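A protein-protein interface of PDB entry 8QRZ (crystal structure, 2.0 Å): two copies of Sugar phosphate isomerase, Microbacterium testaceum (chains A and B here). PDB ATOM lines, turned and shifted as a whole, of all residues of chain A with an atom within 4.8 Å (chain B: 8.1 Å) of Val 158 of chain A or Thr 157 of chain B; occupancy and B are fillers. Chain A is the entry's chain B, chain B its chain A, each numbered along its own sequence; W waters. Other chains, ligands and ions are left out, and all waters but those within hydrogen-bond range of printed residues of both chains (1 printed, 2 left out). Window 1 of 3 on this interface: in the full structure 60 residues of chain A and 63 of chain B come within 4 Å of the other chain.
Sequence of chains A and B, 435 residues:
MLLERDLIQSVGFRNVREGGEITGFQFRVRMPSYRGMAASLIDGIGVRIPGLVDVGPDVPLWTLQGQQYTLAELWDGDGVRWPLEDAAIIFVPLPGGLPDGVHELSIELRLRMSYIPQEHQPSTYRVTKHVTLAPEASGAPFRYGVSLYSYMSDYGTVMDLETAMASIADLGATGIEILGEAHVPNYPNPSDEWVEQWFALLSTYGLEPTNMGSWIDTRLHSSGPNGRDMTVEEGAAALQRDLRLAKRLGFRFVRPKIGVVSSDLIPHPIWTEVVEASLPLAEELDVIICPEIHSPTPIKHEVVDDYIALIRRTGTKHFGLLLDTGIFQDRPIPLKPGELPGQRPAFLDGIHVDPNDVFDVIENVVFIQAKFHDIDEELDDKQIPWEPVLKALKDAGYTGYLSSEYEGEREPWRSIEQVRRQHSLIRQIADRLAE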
ATOM      1  N   LEU A   2      -5.401  18.035 -12.999  1.00  0.00           N
ATOM      2  CA  LEU A   2      -4.392  17.838 -14.021  1.00  0.00           C
ATOM      3  C   LEU A   2      -4.507  16.444 -14.611  1.00  0.00           C
ATOM      4  O   LEU A   2      -5.038  15.518 -13.989  1.00  0.00           O
ATOM      5  CB  LEU A   2      -3.003  18.046 -13.433  1.00  0.00           C
ATOM      6  CG  LEU A   2      -2.847  19.422 -12.791  1.00  0.00           C
ATOM      7  CD1 LEU A   2      -1.811  19.333 -11.710  1.00  0.00           C
ATOM      8  CD2 LEU A   2      -2.477  20.492 -13.840  1.00  0.00           C
ATOM      9  N   LEU A   3      -3.986  16.303 -15.827  1.00  0.00           N
ATOM     10  CA  LEU A   3      -3.946  15.038 -16.544  1.00  0.00           C
ATOM     11  C   LEU A   3      -2.538  14.452 -16.500  1.00  0.00           C
ATOM     12  O   LEU A   3      -1.546  15.183 -16.393  1.00  0.00           O
ATOM     13  CB  LEU A   3      -4.362  15.249 -18.007  1.00  0.00           C
ATOM     14  CG  LEU A   3      -5.768  15.805 -18.133  1.00  0.00           C
ATOM     15  CD1 LEU A   3      -6.036  16.223 -19.574  1.00  0.00           C
ATOM     16  CD2 LEU A   3      -6.769  14.761 -17.649  1.00  0.00           C
ATOM     17  N   GLU A   4      -2.455  13.128 -16.607  1.00  0.00           N
ATOM     18  CA  GLU A   4      -1.154  12.468 -16.656  1.00  0.00           C
ATOM     19  C   GLU A   4      -0.509  12.665 -18.027  1.00  0.00           C
ATOM     20  O   GLU A   4      -1.194  12.849 -19.046  1.00  0.00           O
ATOM     21  CB  GLU A   4      -1.304  10.981 -16.322  1.00  0.00           C
ATOM     22  CG  GLU A   4      -2.230  10.720 -15.069  1.00  0.00           C
ATOM     23  CD  GLU A   4      -2.897   9.306 -15.041  1.00  0.00           C
ATOM     24  OE1 GLU A   4      -2.260   8.322 -15.502  1.00  0.00           O
ATOM     25  OE2 GLU A   4      -4.061   9.199 -14.574  1.00  0.00           O
ATOM     26  N   ARG A   5       0.829  12.633 -18.038  1.00  0.00           N
ATOM     27  CA  ARG A   5       1.594  12.964 -19.239  1.00  0.00           C
ATOM     28  C   ARG A   5       1.356  11.964 -20.369  1.00  0.00           C
ATOM     29  O   ARG A   5       1.119  12.360 -21.521  1.00  0.00           O
ATOM     30  CB  ARG A   5       3.077  13.031 -18.910  1.00  0.00           C
ATOM     31  CG  ARG A   5       3.911  13.745 -19.985  1.00  0.00           C
ATOM     32  CD  ARG A   5       3.503  15.221 -20.104  1.00  0.00           C
ATOM     33  NE  ARG A   5       4.438  16.030 -20.890  1.00  0.00           N
ATOM     34  CZ  ARG A   5       4.798  17.263 -20.559  1.00  0.00           C
ATOM     35  NH1 ARG A   5       4.370  17.835 -19.443  1.00  0.00           N
ATOM     36  NH2 ARG A   5       5.618  17.941 -21.360  1.00  0.00           N
ATOM     37  N   ARG A  30      -5.878  11.720 -22.823  1.00  0.00           N
ATOM     38  CA  ARG A  30      -5.566  13.139 -22.885  1.00  0.00           C
ATOM     39  C   ARG A  30      -5.453  13.585 -24.343  1.00  0.00           C
ATOM     40  O   ARG A  30      -4.709  12.996 -25.126  1.00  0.00           O
ATOM     41  CB  ARG A  30      -4.262  13.412 -22.123  1.00  0.00           C
ATOM     42  CG  ARG A  30      -3.690  14.795 -22.332  1.00  0.00           C
ATOM     43  CD  ARG A  30      -2.496  15.128 -21.375  1.00  0.00           C
ATOM     44  NE  ARG A  30      -1.261  14.507 -21.845  1.00  0.00           N
ATOM     45  CZ  ARG A  30      -0.561  14.914 -22.897  1.00  0.00           C
ATOM     46  NH1 ARG A  30      -0.884  16.014 -23.557  1.00  0.00           N
ATOM     47  NH2 ARG A  30       0.472  14.183 -23.309  1.00  0.00           N
ATOM     48  N   ASP A 154       5.270  14.163  -6.826  1.00  0.00           N
ATOM     49  CA  ASP A 154       4.173  14.426  -7.796  1.00  0.00           C
ATOM     50  C   ASP A 154       3.240  15.466  -7.175  1.00  0.00           C
ATOM     51  O   ASP A 154       2.818  16.378  -7.884  1.00  0.00           O
ATOM     52  CB  ASP A 154       3.405  13.157  -8.176  1.00  0.00           C
ATOM     53  CG  ASP A 154       4.163  12.215  -9.091  1.00  0.00           C
ATOM     54  OD1 ASP A 154       4.948  12.702  -9.911  1.00  0.00           O
ATOM     55  OD2 ASP A 154       3.951  11.002  -8.973  1.00  0.00           O
ATOM     56  N   GLY A 156       1.982  18.624  -5.737  1.00  0.00           N
ATOM     57  CA  GLY A 156       2.507  19.958  -5.841  1.00  0.00           C
ATOM     58  C   GLY A 156       3.293  20.253  -7.106  1.00  0.00           C
ATOM     59  O   GLY A 156       3.670  21.415  -7.317  1.00  0.00           O
ATOM     60  N   THR A 157       3.581  19.247  -7.938  1.00  0.00           N
ATOM     61  CA  THR A 157       4.262  19.469  -9.210  1.00  0.00           C
ATOM     62  C   THR A 157       3.442  19.003 -10.396  1.00  0.00           C
ATOM     63  O   THR A 157       3.328  19.739 -11.389  1.00  0.00           O
ATOM     64  CB  THR A 157       5.651  18.795  -9.259  1.00  0.00           C
ATOM     65  OG1 THR A 157       5.510  17.379  -9.169  1.00  0.00           O
ATOM     66  CG2 THR A 157       6.543  19.298  -8.154  1.00  0.00           C
ATOM     67  N   VAL A 158       2.855  17.804 -10.327  1.00  0.00           N
ATOM     68  CA  VAL A 158       1.959  17.310 -11.365  1.00  0.00           C
ATOM     69  C   VAL A 158       0.588  16.948 -10.811  1.00  0.00           C
ATOM     70  O   VAL A 158      -0.270  16.460 -11.554  1.00  0.00           O
ATOM     71  CB  VAL A 158       2.574  16.113 -12.118  1.00  0.00           C
ATOM     72  CG1 VAL A 158       4.019  16.394 -12.443  1.00  0.00           C
ATOM     73  CG2 VAL A 158       2.434  14.809 -11.326  1.00  0.00           C
ATOM     74  N   MET A 159       0.351  17.206  -9.525  1.00  0.00           N
ATOM     75  CA  MET A 159      -0.826  16.674  -8.877  1.00  0.00           C
ATOM     76  C   MET A 159      -1.318  17.657  -7.841  1.00  0.00           C
ATOM     77  O   MET A 159      -0.526  18.244  -7.115  1.00  0.00           O
ATOM     78  CB  MET A 159      -0.525  15.341  -8.195  1.00  0.00           C
ATOM     79  CG  MET A 159      -1.745  14.491  -8.084  1.00  0.00           C
ATOM     80  SD  MET A 159      -1.369  13.012  -7.176  1.00  0.00           S
ATOM     81  CE  MET A 159      -1.220  11.852  -8.511  1.00  0.00           C
ATOM     82  N   ASP A 160      -2.623  17.838  -7.778  1.00  0.00           N
ATOM     83  CA  ASP A 160      -3.163  18.615  -6.684  1.00  0.00           C
ATOM     84  C   ASP A 160      -4.108  17.702  -5.892  1.00  0.00           C
ATOM     85  O   ASP A 160      -4.227  16.504  -6.169  1.00  0.00           O
ATOM     86  CB  ASP A 160      -3.832  19.881  -7.212  1.00  0.00           C
ATOM     87  CG  ASP A 160      -4.896  19.588  -8.251  1.00  0.00           C
ATOM     88  OD1 ASP A 160      -5.266  18.414  -8.434  1.00  0.00           O
ATOM     89  OD2 ASP A 160      -5.386  20.546  -8.880  1.00  0.00           O
ATOM     90  N   TRP A 413       4.810  10.852 -12.161  1.00  0.00           N
ATOM     91  CA  TRP A 413       3.609  10.040 -12.411  1.00  0.00           C
ATOM     92  C   TRP A 413       3.743   8.564 -12.041  1.00  0.00           C
ATOM     93  O   TRP A 413       2.727   7.873 -11.967  1.00  0.00           O
ATOM     94  CB  TRP A 413       3.126  10.151 -13.882  1.00  0.00           C
ATOM     95  CG  TRP A 413       2.673  11.536 -14.243  1.00  0.00           C
ATOM     96  CD1 TRP A 413       1.447  12.107 -14.016  1.00  0.00           C
ATOM     97  CD2 TRP A 413       3.465  12.529 -14.887  1.00  0.00           C
ATOM     98  NE1 TRP A 413       1.438  13.418 -14.480  1.00  0.00           N
ATOM     99  CE2 TRP A 413       2.668  13.691 -15.022  1.00  0.00           C
ATOM    100  CE3 TRP A 413       4.763  12.542 -15.396  1.00  0.00           C
ATOM    101  CZ2 TRP A 413       3.146  14.851 -15.618  1.00  0.00           C
ATOM    102  CZ3 TRP A 413       5.235  13.695 -15.981  1.00  0.00           C
ATOM    103  CH2 TRP A 413       4.432  14.836 -16.089  1.00  0.00           C
ATOM    104  N   LEU B   2       1.685  25.587  -9.299  1.00  0.00           N
ATOM    105  CA  LEU B   2       2.499  24.353  -9.278  1.00  0.00           C
ATOM    106  C   LEU B   2       3.999  24.660  -9.296  1.00  0.00           C
ATOM    107  O   LEU B   2       4.384  25.698  -9.832  1.00  0.00           O
ATOM    108  CB  LEU B   2       2.079  23.487 -10.465  1.00  0.00           C
ATOM    109  CG  LEU B   2       0.688  22.869 -10.352  1.00  0.00           C
ATOM    110  CD1 LEU B   2       0.215  22.361 -11.698  1.00  0.00           C
ATOM    111  CD2 LEU B   2       0.671  21.755  -9.322  1.00  0.00           C
ATOM    112  N   LEU B   3       4.783  23.782  -8.688  1.00  0.00           N
ATOM    113  CA  LEU B   3       6.232  23.922  -8.627  1.00  0.00           C
ATOM    114  C   LEU B   3       6.884  23.005  -9.653  1.00  0.00           C
ATOM    115  O   LEU B   3       6.350  21.941  -9.987  1.00  0.00           O
ATOM    116  CB  LEU B   3       6.756  23.582  -7.218  1.00  0.00           C
ATOM    117  CG  LEU B   3       6.306  24.584  -6.152  1.00  0.00           C
ATOM    118  CD1 LEU B   3       6.646  24.135  -4.725  1.00  0.00           C
ATOM    119  CD2 LEU B   3       6.875  25.969  -6.443  1.00  0.00           C
ATOM    120  N   GLU B   4       8.047  23.435 -10.146  1.00  0.00           N
ATOM    121  CA  GLU B   4       8.838  22.642 -11.077  1.00  0.00           C
ATOM    122  C   GLU B   4       9.467  21.440 -10.369  1.00  0.00           C
ATOM    123  O   GLU B   4       9.734  21.462  -9.159  1.00  0.00           O
ATOM    124  CB  GLU B   4       9.909  23.529 -11.744  1.00  0.00           C
ATOM    125  CG  GLU B   4       9.323  24.859 -12.264  1.00  0.00           C
ATOM    126  CD  GLU B   4      10.376  25.952 -12.629  1.00  0.00           C
ATOM    127  OE1 GLU B   4      11.571  25.627 -12.832  1.00  0.00           O
ATOM    128  OE2 GLU B   4       9.992  27.146 -12.692  1.00  0.00           O
ATOM    129  N   ARG B   5       9.692  20.374 -11.144  1.00  0.00           N
ATOM    130  CA  ARG B   5      10.237  19.136 -10.592  1.00  0.00           C
ATOM    131  C   ARG B   5      11.639  19.340 -10.019  1.00  0.00           C
ATOM    132  O   ARG B   5      11.958  18.849  -8.925  1.00  0.00           O
ATOM    133  CB  ARG B   5      10.249  18.049 -11.670  1.00  0.00           C
ATOM    134  CG  ARG B   5      10.290  16.621 -11.096  1.00  0.00           C
ATOM    135  CD  ARG B   5       9.100  16.365 -10.158  1.00  0.00           C
ATOM    136  NE  ARG B   5       8.956  14.957  -9.790  1.00  0.00           N
ATOM    137  CZ  ARG B   5       7.817  14.274  -9.805  1.00  0.00           C
ATOM    138  NH1 ARG B   5       6.673  14.838 -10.165  1.00  0.00           N
ATOM    139  NH2 ARG B   5       7.821  12.998  -9.429  1.00  0.00           N
ATOM    140  N   TYR B 151       3.979  26.305 -23.994  1.00  0.00           N
ATOM    141  CA  TYR B 151       3.894  25.350 -22.890  1.00  0.00           C
ATOM    142  C   TYR B 151       2.967  24.176 -23.201  1.00  0.00           C
ATOM    143  O   TYR B 151       2.463  23.531 -22.276  1.00  0.00           O
ATOM    144  CB  TYR B 151       3.413  26.039 -21.609  1.00  0.00           C
ATOM    145  CG  TYR B 151       4.280  27.173 -21.116  1.00  0.00           C
ATOM    146  CD1 TYR B 151       5.671  27.096 -21.180  1.00  0.00           C
ATOM    147  CD2 TYR B 151       3.710  28.317 -20.566  1.00  0.00           C
ATOM    148  CE1 TYR B 151       6.466  28.126 -20.725  1.00  0.00           C
ATOM    149  CE2 TYR B 151       4.509  29.365 -20.107  1.00  0.00           C
ATOM    150  CZ  TYR B 151       5.880  29.263 -20.192  1.00  0.00           C
ATOM    151  OH  TYR B 151       6.679  30.292 -19.745  1.00  0.00           O
ATOM    152  N   MET B 152       2.685  23.925 -24.481  1.00  0.00           N
ATOM    153  CA  MET B 152       1.922  22.754 -24.884  1.00  0.00           C
ATOM    154  C   MET B 152       2.493  21.493 -24.253  1.00  0.00           C
ATOM    155  O   MET B 152       3.710  21.327 -24.167  1.00  0.00           O
ATOM    156  CB  MET B 152       1.943  22.596 -26.401  1.00  0.00           C
ATOM    157  CG  MET B 152       1.396  21.258 -26.893  1.00  0.00           C
ATOM    158  SD  MET B 152       1.908  20.898 -28.576  1.00  0.00           S
ATOM    159  CE  MET B 152       1.202  19.255 -28.762  1.00  0.00           C
ATOM    160  N   SER B 153       1.581  20.590 -23.860  1.00  0.00           N
ATOM    161  CA  SER B 153       1.804  19.349 -23.118  1.00  0.00           C
ATOM    162  C   SER B 153       2.083  19.646 -21.639  1.00  0.00           C
ATOM    163  O   SER B 153       1.472  19.021 -20.765  1.00  0.00           O
ATOM    164  CB  SER B 153       2.905  18.492 -23.754  1.00  0.00           C
ATOM    165  OG  SER B 153       2.602  18.229 -25.122  1.00  0.00           O
ATOM    166  N   ASP B 154       2.961  20.606 -21.340  1.00  0.00           N
ATOM    167  CA  ASP B 154       3.108  21.070 -19.960  1.00  0.00           C
ATOM    168  C   ASP B 154       1.788  21.589 -19.420  1.00  0.00           C
ATOM    169  O   ASP B 154       1.356  21.203 -18.327  1.00  0.00           O
ATOM    170  CB  ASP B 154       4.184  22.162 -19.865  1.00  0.00           C
ATOM    171  CG  ASP B 154       5.578  21.589 -19.932  1.00  0.00           C
ATOM    172  OD1 ASP B 154       5.695  20.401 -19.552  1.00  0.00           O
ATOM    173  OD2 ASP B 154       6.545  22.301 -20.347  1.00  0.00           O
ATOM    174  N   TYR B 155       1.125  22.454 -20.187  1.00  0.00           N
ATOM    175  CA  TYR B 155      -0.131  23.051 -19.764  1.00  0.00           C
ATOM    176  C   TYR B 155      -1.190  21.980 -19.567  1.00  0.00           C
ATOM    177  O   TYR B 155      -1.505  21.229 -20.492  1.00  0.00           O
ATOM    178  CB  TYR B 155      -0.614  24.072 -20.803  1.00  0.00           C
ATOM    179  CG  TYR B 155      -1.615  25.039 -20.236  1.00  0.00           C
ATOM    180  CD1 TYR B 155      -1.194  26.152 -19.531  1.00  0.00           C
ATOM    181  CD2 TYR B 155      -2.980  24.828 -20.368  1.00  0.00           C
ATOM    182  CE1 TYR B 155      -2.104  27.053 -18.989  1.00  0.00           C
ATOM    183  CE2 TYR B 155      -3.899  25.729 -19.817  1.00  0.00           C
ATOM    184  CZ  TYR B 155      -3.439  26.836 -19.135  1.00  0.00           C
ATOM    185  OH  TYR B 155      -4.305  27.760 -18.575  1.00  0.00           O
ATOM    186  N   GLY B 156      -1.761  21.929 -18.377  1.00  0.00           N
ATOM    187  CA  GLY B 156      -2.728  20.901 -18.044  1.00  0.00           C
ATOM    188  C   GLY B 156      -2.169  19.605 -17.478  1.00  0.00           C
ATOM    189  O   GLY B 156      -2.959  18.754 -17.054  1.00  0.00           O
ATOM    190  N   THR B 157      -0.850  19.398 -17.487  1.00  0.00           N
ATOM    191  CA  THR B 157      -0.250  18.248 -16.814  1.00  0.00           C
ATOM    192  C   THR B 157       0.653  18.662 -15.662  1.00  0.00           C
ATOM    193  O   THR B 157       0.586  18.070 -14.588  1.00  0.00           O
ATOM    194  CB  THR B 157       0.556  17.360 -17.763  1.00  0.00           C
ATOM    195  OG1 THR B 157       1.681  18.085 -18.276  1.00  0.00           O
ATOM    196  CG2 THR B 157      -0.310  16.820 -18.910  1.00  0.00           C
ATOM    197  N   VAL B 158       1.515  19.650 -15.883  1.00  0.00           N
ATOM    198  CA  VAL B 158       2.352  20.227 -14.839  1.00  0.00           C
ATOM    199  C   VAL B 158       2.113  21.720 -14.655  1.00  0.00           C
ATOM    200  O   VAL B 158       2.672  22.313 -13.721  1.00  0.00           O
ATOM    201  CB  VAL B 158       3.847  19.970 -15.127  1.00  0.00           C
ATOM    202  CG1 VAL B 158       4.079  18.482 -15.446  1.00  0.00           C
ATOM    203  CG2 VAL B 158       4.318  20.850 -16.290  1.00  0.00           C
ATOM    204  N   MET B 159       1.302  22.351 -15.494  1.00  0.00           N
ATOM    205  CA  MET B 159       1.182  23.800 -15.506  1.00  0.00           C
ATOM    206  C   MET B 159      -0.287  24.186 -15.510  1.00  0.00           C
ATOM    207  O   MET B 159      -1.085  23.554 -16.201  1.00  0.00           O
ATOM    208  CB  MET B 159       1.885  24.354 -16.772  1.00  0.00           C
ATOM    209  CG  MET B 159       1.863  25.855 -16.911  1.00  0.00           C
ATOM    210  SD  MET B 159       3.333  26.436 -17.749  1.00  0.00           S
ATOM    211  CE  MET B 159       4.619  25.558 -16.861  1.00  0.00           C
ATOM    212  N   ASP B 160      -0.665  25.190 -14.723  1.00  0.00           N
ATOM    213  CA  ASP B 160      -1.990  25.783 -14.865  1.00  0.00           C
ATOM    214  C   ASP B 160      -1.830  27.252 -15.259  1.00  0.00           C
ATOM    215  O   ASP B 160      -0.716  27.737 -15.429  1.00  0.00           O
ATOM    216  CB  ASP B 160      -2.835  25.621 -13.601  1.00  0.00           C
ATOM    217  CG  ASP B 160      -2.194  26.230 -12.372  1.00  0.00           C
ATOM    218  OD1 ASP B 160      -1.094  26.776 -12.475  1.00  0.00           O
ATOM    219  OD2 ASP B 160      -2.809  26.161 -11.294  1.00  0.00           O
ATOM    220  N   ARG B 410       8.987  18.325 -26.327  1.00  0.00           N
ATOM    221  CA  ARG B 410       8.016  18.571 -25.259  1.00  0.00           C
ATOM    222  C   ARG B 410       8.295  17.692 -24.044  1.00  0.00           C
ATOM    223  O   ARG B 410       7.406  17.030 -23.510  1.00  0.00           O
ATOM    224  CB  ARG B 410       6.607  18.345 -25.776  1.00  0.00           C
ATOM    225  CG  ARG B 410       6.324  19.066 -27.072  1.00  0.00           C
ATOM    226  CD  ARG B 410       5.989  20.470 -26.763  1.00  0.00           C
ATOM    227  NE  ARG B 410       5.668  21.273 -27.932  1.00  0.00           N
ATOM    228  CZ  ARG B 410       5.583  22.589 -27.870  1.00  0.00           C
ATOM    229  NH1 ARG B 410       5.860  23.239 -26.751  1.00  0.00           N
ATOM    230  NH2 ARG B 410       5.207  23.272 -28.946  1.00  0.00           N
ATOM    231  N   PRO B 412       8.764  17.189 -20.234  1.00  0.00           N
ATOM    232  CA  PRO B 412       8.127  17.933 -19.143  1.00  0.00           C
ATOM    233  C   PRO B 412       9.059  18.965 -18.533  1.00  0.00           C
ATOM    234  O   PRO B 412      10.232  18.691 -18.265  1.00  0.00           O
ATOM    235  CB  PRO B 412       7.764  16.827 -18.152  1.00  0.00           C
ATOM    236  CG  PRO B 412       7.415  15.675 -19.105  1.00  0.00           C
ATOM    237  CD  PRO B 412       8.450  15.750 -20.181  1.00  0.00           C
ATOM    238  N   TRP B 413       8.524  20.174 -18.361  1.00  0.00           N
ATOM    239  CA  TRP B 413       9.199  21.352 -17.811  1.00  0.00           C
ATOM    240  C   TRP B 413      10.219  21.945 -18.782  1.00  0.00           C
ATOM    241  O   TRP B 413      10.637  23.084 -18.579  1.00  0.00           O
ATOM    242  CB  TRP B 413       9.865  21.062 -16.428  1.00  0.00           C
ATOM    243  CG  TRP B 413       8.837  20.740 -15.401  1.00  0.00           C
ATOM    244  CD1 TRP B 413       7.995  21.616 -14.781  1.00  0.00           C
ATOM    245  CD2 TRP B 413       8.501  19.445 -14.907  1.00  0.00           C
ATOM    246  NE1 TRP B 413       7.141  20.938 -13.930  1.00  0.00           N
ATOM    247  CE2 TRP B 413       7.440  19.606 -13.988  1.00  0.00           C
ATOM    248  CE3 TRP B 413       9.002  18.158 -15.140  1.00  0.00           C
ATOM    249  CZ2 TRP B 413       6.867  18.528 -13.304  1.00  0.00           C
ATOM    250  CZ3 TRP B 413       8.419  17.090 -14.474  1.00  0.00           C
ATOM    251  CH2 TRP B 413       7.360  17.284 -13.574  1.00  0.00           C
HETATM  252  O   HOH W   1       5.075  15.073 -23.309  1.00  0.00           O
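Water W1 bridges NE of Arg 5 of chain A (2.7 Å) and O of Arg 410 of chain B (3.1 Å).
Leu 2 of chain A touches its own counterpart, Leu 2 of chain B.
Leu 3 of chain A touches Gly 156 of chain B, and with the chains exchanged Gly 156 of chain A touches Leu 3 of chain B.
Arg 5 of chain A touches Asp 154 of chain B, and with the chains exchanged Asp 154 of chain A touches Arg 5 of chain B.
Thr 157 of chain A touches Glu 4 of chain B, but with the chains exchanged Glu 4 of chain A does not touch Thr 157 of chain B (4.1 Å).
Of the 24 pairs that touch across the chains among the printed residues, 18 have their exchanged pair printed and touching as well.
Val 158 of chain A touches four residues of chain B.
Printed residues of chain A within 4 Å of Arg 410 of chain B: Arg 5.
Printed residues of chain A within 4 Å of Gly 156 of chain B: Leu 2 and Leu 3.
Of the printed residues of chain A, Trp 413 of chain B touches Val 158.
Glu 4 of chain A touches none of the printed residues of chain B.
Met 159 of chain A touches none of the printed residues of chain B.
The nearest residue of chain A that does not touch Thr 157 of chain B is Glu 4 of chain A (4.1 Å).
Of the 17 printed residues of chain B, 12 touch a printed residue of chain A.
Hydrophobic or aromatic side chains of chain B that line the printed part of chain A: Leu 2, Leu 3, Val 158, Pro 412 and Trp 413.
Printed residues of chain A that touch a printed residue of chain B: Leu 2, Leu 3, Arg 5, Arg 30, Asp 154, Gly 156, Thr 157, Val 158 and Trp 413.
Hydrophobic or aromatic side chains of chain A that line the printed part of chain B: Leu 2, Leu 3, Val 158 and Trp 413.
Along chain A the printed residues that touch a printed residue of chain B span positions 2 to 413.
The side-chain hydroxyl of Thr 157 of chain A is in hydrogen-bond range of the guanidinium group of Arg 5 of chain B.
O of Gly 156 of chain A lies within hydrogen-bond range of N of Leu 3 of chain B (3.0 Å).
The backbone carbonyl oxygen (O) of Ser 153 of chain B sits at hydrogen-bond distance from the guanidinium group (NH1) of Arg 5 of chain A (3.4 Å).
The guanidinium group (NH2) of Arg 5 of chain A lies close to the backbone nitrogen (N) of Pro 412 of chain B (3.4 Å).
The backbone carbonyl oxygen (O) of Arg 410 of chain B is in hydrogen-bond range of the guanidinium group (NH2) of Arg 5 of chain A (2.9 Å).
OD1 of Asp 154 of chain B is in salt-bridge range of NH1 of Arg 5 of chain A (2.9 Å).
The side-chain hydroxyl (OG1) of Thr 157 of chain B lies within hydrogen-bond range of the guanidinium group (NH1) of Arg 5 of chain A, at 2.9 Å.
The backbone carbonyl oxygen (O) of Gly 156 of chain B is in hydrogen-bond range of the backbone NH (N) of Leu 3 of chain A, 2.9 Å away.
The guanidinium group of Arg 5 of chain B is in salt-bridge range of the side-chain carboxylate of Asp 154 of chain A, at 2.8 Å.
O of Asp 154 of chain B lies within hydrogen-bond range of OG1 of Thr 157 of chain B, at 3.1 Å.
OD1 of Asp 154 of chain B lies within hydrogen-bond range of N of Trp 413 of chain B, 3.1 Å away.
O of Glu 4 of chain A is in hydrogen-bond range of NE of Arg 30 of chain A, 3.3 Å away.
The backbone carbonyl oxygen (O) of Arg 5 of chain A is in hydrogen-bond range of the guanidinium group (NH2) of Arg 30 of chain A, at 2.6 Å.
N of Met 159 of chain B lies within hydrogen-bond range of O of Asp 154 of chain B, 3.1 Å away.
OG1 of Thr 157 of chain B is in hydrogen-bond range of O of Ser 153 of chain B.
Among the printed residues, merely in contact across the chains: Leu 2 of chain A with Leu 2 of chain B (3.6 Å), Leu 2 of chain A with Gly 156 of chain B (3.5 Å), Leu 2 of chain A with Thr 157 of chain B (3.8 Å), Leu 3 of chain A with Thr 157 of chain B (3.2 Å), Arg 30 of chain A with Thr 157 of chain B (3.7 Å), Gly 156 of chain A with Leu 2 of chain B (3.6 Å), Thr 157 of chain A with Leu 2 of chain B (3.9 Å), Thr 157 of chain A with Leu 3 of chain B (3.2 Å), Thr 157 of chain A with Glu 4 of chain B (3.98 Å), Thr 157 of chain A with Val 158 of chain B (3.5 Å), Val 158 of chain A with Arg 5 of chain B (3.8 Å), Val 158 of chain A with Thr 157 of chain B (3.5 Å), Val 158 of chain A with Val 158 of chain B (3.7 Å), Val 158 of chain A with Trp 413 of chain B (3.6 Å) and Trp 413 of chain A with Val 158 of chain B (3.7 Å).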
